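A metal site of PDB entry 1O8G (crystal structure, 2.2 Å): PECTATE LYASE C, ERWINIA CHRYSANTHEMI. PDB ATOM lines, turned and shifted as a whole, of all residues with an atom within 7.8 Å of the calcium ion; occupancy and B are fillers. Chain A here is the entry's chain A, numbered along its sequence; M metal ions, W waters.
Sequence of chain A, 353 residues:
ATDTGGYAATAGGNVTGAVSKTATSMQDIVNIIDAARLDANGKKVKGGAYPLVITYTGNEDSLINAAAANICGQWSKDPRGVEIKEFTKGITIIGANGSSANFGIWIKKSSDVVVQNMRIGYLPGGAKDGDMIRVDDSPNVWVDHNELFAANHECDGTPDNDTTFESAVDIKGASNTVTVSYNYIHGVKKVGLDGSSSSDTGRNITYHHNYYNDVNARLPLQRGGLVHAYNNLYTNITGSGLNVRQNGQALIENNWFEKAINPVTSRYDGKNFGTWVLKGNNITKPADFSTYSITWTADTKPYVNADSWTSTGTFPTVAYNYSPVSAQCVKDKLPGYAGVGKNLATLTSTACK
The calcium ion is bound by the side-chain carboxylate (OE1) of Glu 166 (2.2 Å), the side-chain carboxylate (OD2) of Asp 131 (2.3 Å), water W1 (2.4 Å), the side-chain carboxylate (OD1) of Asp 129 (2.4 Å), the side-chain carboxylate (OD1) of Asp 131 (2.4 Å), the side-chain carboxylate (OD2) of Asp 170 (2.4 Å) and water W2 (2.6 Å). The calcium ion has seven donor atoms within binding distance.
OD1 of Asp 170 lies close to OG of Ser 167 (3.2 Å). OD2 of Asp 129 lies within salt-bridge range of NH1 of Arg 134, 2.9 Å away. The side-chain carboxylate (OD1) of Asp 170 lies within hydrogen-bond range of the backbone NH (N) of Leu 193 (2.8 Å). O of Ile 133 is in hydrogen-bond range of N of Asp 170. NZ of Lys 190 is in salt-bridge range of OE2 of Glu 166, 2.7 Å away. The side-chain carboxylate (OE1) of Glu 166 lies close to the side-chain hydroxyl (OG) of Ser 167 (3.3 Å). N of Ser 167 sits close to OD1 of Asp 131. The backbone carbonyl oxygen (O) of Asp 131 sits at hydrogen-bond distance from the indole nitrogen (NE1) of Trp 106 (2.8 Å).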
ATOM      1  N   TRP A 106       6.674  15.365  13.930  1.00  0.00           N
ATOM      2  CA  TRP A 106       5.355  15.303  13.325  1.00  0.00           C
ATOM      3  C   TRP A 106       5.325  16.115  12.034  1.00  0.00           C
ATOM      4  O   TRP A 106       5.397  17.330  12.053  1.00  0.00           O
ATOM      5  CB  TRP A 106       4.308  15.810  14.308  1.00  0.00           C
ATOM      6  CG  TRP A 106       4.390  15.100  15.633  1.00  0.00           C
ATOM      7  CD1 TRP A 106       4.749  13.800  15.834  1.00  0.00           C
ATOM      8  CD2 TRP A 106       4.112  15.644  16.927  1.00  0.00           C
ATOM      9  NE1 TRP A 106       4.723  13.508  17.164  1.00  0.00           N
ATOM     10  CE2 TRP A 106       4.342  14.613  17.858  1.00  0.00           C
ATOM     11  CE3 TRP A 106       3.709  16.897  17.381  1.00  0.00           C
ATOM     12  CZ2 TRP A 106       4.163  14.799  19.223  1.00  0.00           C
ATOM     13  CZ3 TRP A 106       3.529  17.083  18.747  1.00  0.00           C
ATOM     14  CH2 TRP A 106       3.762  16.043  19.651  1.00  0.00           C
ATOM     15  N   GLY A 126       1.142   9.313  25.340  1.00  0.00           N
ATOM     16  CA  GLY A 126       0.564   8.298  24.489  1.00  0.00           C
ATOM     17  C   GLY A 126      -0.933   8.482  24.328  1.00  0.00           C
ATOM     18  O   GLY A 126      -1.500   8.122  23.295  1.00  0.00           O
ATOM     19  N   LYS A 128      -2.366  11.330  24.136  1.00  0.00           N
ATOM     20  CA  LYS A 128      -2.578  12.547  23.351  1.00  0.00           C
ATOM     21  C   LYS A 128      -1.793  12.574  22.043  1.00  0.00           C
ATOM     22  O   LYS A 128      -1.267  13.615  21.623  1.00  0.00           O
ATOM     23  CB  LYS A 128      -2.307  13.807  24.198  1.00  0.00           C
ATOM     24  CG  LYS A 128      -3.255  13.975  25.366  1.00  0.00           C
ATOM     25  CD  LYS A 128      -2.977  15.237  26.124  1.00  0.00           C
ATOM     26  CE  LYS A 128      -3.694  15.223  27.464  1.00  0.00           C
ATOM     27  NZ  LYS A 128      -3.148  14.164  28.357  1.00  0.00           N
ATOM     28  N   ASP A 129      -1.724  11.412  21.398  1.00  0.00           N
ATOM     29  CA  ASP A 129      -1.059  11.242  20.116  1.00  0.00           C
ATOM     30  C   ASP A 129       0.429  11.527  20.120  1.00  0.00           C
ATOM     31  O   ASP A 129       0.936  12.172  19.202  1.00  0.00           O
ATOM     32  CB  ASP A 129      -1.759  12.085  19.044  1.00  0.00           C
ATOM     33  CG  ASP A 129      -1.781  11.424  17.676  1.00  0.00           C
ATOM     34  OD1 ASP A 129      -1.606  10.187  17.597  1.00  0.00           O
ATOM     35  OD2 ASP A 129      -2.015  12.130  16.673  1.00  0.00           O
ATOM     36  N   GLY A 130       1.133  11.032  21.118  1.00  0.00           N
ATOM     37  CA  GLY A 130       2.561  11.258  21.179  1.00  0.00           C
ATOM     38  C   GLY A 130       3.357  10.306  20.299  1.00  0.00           C
ATOM     39  O   GLY A 130       4.144   9.529  20.797  1.00  0.00           O
ATOM     40  N   ASP A 131       3.155  10.386  18.983  1.00  0.00           N
ATOM     41  CA  ASP A 131       3.868   9.538  18.042  1.00  0.00           C
ATOM     42  C   ASP A 131       5.338   9.901  17.962  1.00  0.00           C
ATOM     43  O   ASP A 131       5.692  11.067  18.148  1.00  0.00           O
ATOM     44  CB  ASP A 131       3.294   9.703  16.644  1.00  0.00           C
ATOM     45  CG  ASP A 131       1.888   9.196  16.535  1.00  0.00           C
ATOM     46  OD1 ASP A 131       1.554   8.189  17.185  1.00  0.00           O
ATOM     47  OD2 ASP A 131       1.109   9.802  15.787  1.00  0.00           O
ATOM     48  N   MET A 132       6.183   8.914  17.690  1.00  0.00           N
ATOM     49  CA  MET A 132       7.626   9.137  17.546  1.00  0.00           C
ATOM     50  C   MET A 132       7.829   9.813  16.213  1.00  0.00           C
ATOM     51  O   MET A 132       8.567  10.801  16.101  1.00  0.00           O
ATOM     52  CB  MET A 132       8.387   7.818  17.626  1.00  0.00           C
ATOM     53  CG  MET A 132       8.234   7.132  18.967  1.00  0.00           C
ATOM     54  SD  MET A 132       9.350   5.750  19.208  1.00  0.00           S
ATOM     55  CE  MET A 132       8.159   4.400  19.358  1.00  0.00           C
ATOM     56  N   ILE A 133       7.130   9.305  15.198  1.00  0.00           N
ATOM     57  CA  ILE A 133       7.149   9.875  13.858  1.00  0.00           C
ATOM     58  C   ILE A 133       5.750   9.794  13.251  1.00  0.00           C
ATOM     59  O   ILE A 133       5.099   8.746  13.322  1.00  0.00           O
ATOM     60  CB  ILE A 133       8.201   9.196  12.941  1.00  0.00           C
ATOM     61  CG1 ILE A 133       9.597   9.685  13.358  1.00  0.00           C
ATOM     62  CG2 ILE A 133       7.960   9.577  11.478  1.00  0.00           C
ATOM     63  CD1 ILE A 133      10.684   9.273  12.438  1.00  0.00           C
ATOM     64  N   ARG A 134       5.252  10.918  12.758  1.00  0.00           N
ATOM     65  CA  ARG A 134       3.939  10.952  12.125  1.00  0.00           C
ATOM     66  C   ARG A 134       4.064  11.609  10.768  1.00  0.00           C
ATOM     67  O   ARG A 134       4.710  12.655  10.638  1.00  0.00           O
ATOM     68  CB  ARG A 134       2.935  11.711  12.985  1.00  0.00           C
ATOM     69  CG  ARG A 134       1.542  11.579  12.498  1.00  0.00           C
ATOM     70  CD  ARG A 134       0.558  11.953  13.572  1.00  0.00           C
ATOM     71  NE  ARG A 134       0.699  13.322  14.040  1.00  0.00           N
ATOM     72  CZ  ARG A 134       0.797  13.662  15.318  1.00  0.00           C
ATOM     73  NH1 ARG A 134       0.789  12.741  16.253  1.00  0.00           N
ATOM     74  NH2 ARG A 134       0.832  14.938  15.664  1.00  0.00           N
ATOM     75  N   GLU A 166       2.221   5.742  22.131  1.00  0.00           N
ATOM     76  CA  GLU A 166       1.643   5.873  20.817  1.00  0.00           C
ATOM     77  C   GLU A 166       2.535   5.150  19.802  1.00  0.00           C
ATOM     78  O   GLU A 166       3.382   4.348  20.186  1.00  0.00           O
ATOM     79  CB  GLU A 166       1.416   7.338  20.437  1.00  0.00           C
ATOM     80  CG  GLU A 166      -0.062   7.689  20.287  1.00  0.00           C
ATOM     81  CD  GLU A 166      -0.796   6.817  19.245  1.00  0.00           C
ATOM     82  OE1 GLU A 166      -0.674   7.044  18.032  1.00  0.00           O
ATOM     83  OE2 GLU A 166      -1.511   5.894  19.666  1.00  0.00           O
ATOM     84  N   SER A 167       2.403   5.489  18.525  1.00  0.00           N
ATOM     85  CA  SER A 167       3.125   4.792  17.473  1.00  0.00           C
ATOM     86  C   SER A 167       4.545   5.173  17.094  1.00  0.00           C
ATOM     87  O   SER A 167       5.024   6.240  17.447  1.00  0.00           O
ATOM     88  CB  SER A 167       2.249   4.789  16.246  1.00  0.00           C
ATOM     89  OG  SER A 167       0.925   4.450  16.651  1.00  0.00           O
ATOM     90  N   ALA A 168       5.213   4.257  16.422  1.00  0.00           N
ATOM     91  CA  ALA A 168       6.578   4.484  15.959  1.00  0.00           C
ATOM     92  C   ALA A 168       6.555   5.331  14.687  1.00  0.00           C
ATOM     93  O   ALA A 168       7.237   6.355  14.626  1.00  0.00           O
ATOM     94  CB  ALA A 168       7.282   3.164  15.707  1.00  0.00           C
ATOM     95  N   VAL A 169       5.811   4.901  13.667  1.00  0.00           N
ATOM     96  CA  VAL A 169       5.712   5.653  12.409  1.00  0.00           C
ATOM     97  C   VAL A 169       4.289   5.588  11.855  1.00  0.00           C
ATOM     98  O   VAL A 169       3.959   4.690  11.088  1.00  0.00           O
ATOM     99  CB  VAL A 169       6.679   5.136  11.281  1.00  0.00           C
ATOM    100  CG1 VAL A 169       6.606   6.073  10.067  1.00  0.00           C
ATOM    101  CG2 VAL A 169       8.125   5.079  11.770  1.00  0.00           C
ATOM    102  N   ASP A 170       3.436   6.535  12.265  1.00  0.00           N
ATOM    103  CA  ASP A 170       2.062   6.574  11.780  1.00  0.00           C
ATOM    104  C   ASP A 170       2.001   7.375  10.505  1.00  0.00           C
ATOM    105  O   ASP A 170       2.561   8.462  10.429  1.00  0.00           O
ATOM    106  CB  ASP A 170       1.142   7.236  12.818  1.00  0.00           C
ATOM    107  CG  ASP A 170       0.507   6.215  13.756  1.00  0.00           C
ATOM    108  OD1 ASP A 170       0.650   5.006  13.532  1.00  0.00           O
ATOM    109  OD2 ASP A 170      -0.171   6.634  14.718  1.00  0.00           O
ATOM    110  N   ILE A 171       1.334   6.833   9.495  1.00  0.00           N
ATOM    111  CA  ILE A 171       1.193   7.507   8.206  1.00  0.00           C
ATOM    112  C   ILE A 171      -0.300   7.656   7.878  1.00  0.00           C
ATOM    113  O   ILE A 171      -1.051   6.698   7.994  1.00  0.00           O
ATOM    114  CB  ILE A 171       1.898   6.695   7.068  1.00  0.00           C
ATOM    115  CG1 ILE A 171       3.411   6.612   7.341  1.00  0.00           C
ATOM    116  CG2 ILE A 171       1.584   7.334   5.684  1.00  0.00           C
ATOM    117  CD1 ILE A 171       4.128   5.490   6.594  1.00  0.00           C
ATOM    118  N   LYS A 172      -0.733   8.856   7.530  1.00  0.00           N
ATOM    119  CA  LYS A 172      -2.138   9.051   7.196  1.00  0.00           C
ATOM    120  C   LYS A 172      -2.330  10.171   6.213  1.00  0.00           C
ATOM    121  O   LYS A 172      -1.388  10.892   5.874  1.00  0.00           O
ATOM    122  CB  LYS A 172      -2.966   9.287   8.451  1.00  0.00           C
ATOM    123  CG  LYS A 172      -2.656  10.548   9.175  1.00  0.00           C
ATOM    124  CD  LYS A 172      -3.620  10.656  10.345  1.00  0.00           C
ATOM    125  CE  LYS A 172      -3.405  11.891  11.165  1.00  0.00           C
ATOM    126  NZ  LYS A 172      -4.381  11.923  12.282  1.00  0.00           N
ATOM    127  N   LYS A 190       2.226  -0.530  19.190  1.00  0.00           N
ATOM    128  CA  LYS A 190       1.577  -0.132  17.938  1.00  0.00           C
ATOM    129  C   LYS A 190       2.603   0.528  17.047  1.00  0.00           C
ATOM    130  O   LYS A 190       2.898   1.700  17.211  1.00  0.00           O
ATOM    131  CB  LYS A 190       0.458   0.864  18.227  1.00  0.00           C
ATOM    132  CG  LYS A 190      -0.675   0.249  19.035  1.00  0.00           C
ATOM    133  CD  LYS A 190      -1.114   1.173  20.141  1.00  0.00           C
ATOM    134  CE  LYS A 190      -1.561   2.494  19.585  1.00  0.00           C
ATOM    135  NZ  LYS A 190      -1.829   3.389  20.715  1.00  0.00           N
ATOM    136  N   GLY A 192       2.741   1.225  13.507  1.00  0.00           N
ATOM    137  CA  GLY A 192       2.323   2.297  12.637  1.00  0.00           C
ATOM    138  C   GLY A 192       1.140   2.010  11.734  1.00  0.00           C
ATOM    139  O   GLY A 192       0.986   0.915  11.197  1.00  0.00           O
ATOM    140  N   LEU A 193       0.333   3.046  11.557  1.00  0.00           N
ATOM    141  CA  LEU A 193      -0.840   3.001  10.717  1.00  0.00           C
ATOM    142  C   LEU A 193      -0.430   3.346   9.316  1.00  0.00           C
ATOM    143  O   LEU A 193       0.611   3.967   9.098  1.00  0.00           O
ATOM    144  CB  LEU A 193      -1.824   4.091  11.153  1.00  0.00           C
ATOM    145  CG  LEU A 193      -2.491   3.904  12.504  1.00  0.00           C
ATOM    146  CD1 LEU A 193      -3.203   5.179  12.902  1.00  0.00           C
ATOM    147  CD2 LEU A 193      -3.455   2.741  12.411  1.00  0.00           C
ATOM    148  N   ARG A 218       0.593  -3.890  13.812  1.00  0.00           N
ATOM    149  CA  ARG A 218       0.620  -2.849  12.783  1.00  0.00           C
ATOM    150  C   ARG A 218       1.974  -2.652  12.076  1.00  0.00           C
ATOM    151  O   ARG A 218       2.610  -1.605  12.219  1.00  0.00           O
ATOM    152  CB  ARG A 218       0.142  -1.528  13.373  1.00  0.00           C
ATOM    153  CG  ARG A 218      -1.169  -1.628  14.100  1.00  0.00           C
ATOM    154  CD  ARG A 218      -1.563  -0.287  14.625  1.00  0.00           C
ATOM    155  NE  ARG A 218      -2.833  -0.365  15.319  1.00  0.00           N
ATOM    156  CZ  ARG A 218      -3.414   0.675  15.925  1.00  0.00           C
ATOM    157  NH1 ARG A 218      -2.835   1.875  15.899  1.00  0.00           N
ATOM    158  NH2 ARG A 218      -4.573   0.516  16.535  1.00  0.00           N
HETATM  159 CA    CA M   1      -0.676   8.412  16.280  1.00  0.00          CA
HETATM  160  O   HOH W   1      -1.516   9.639  14.420  1.00  0.00           O
HETATM  161  O   HOH W   2      -3.099   7.340  16.272  1.00  0.00           O
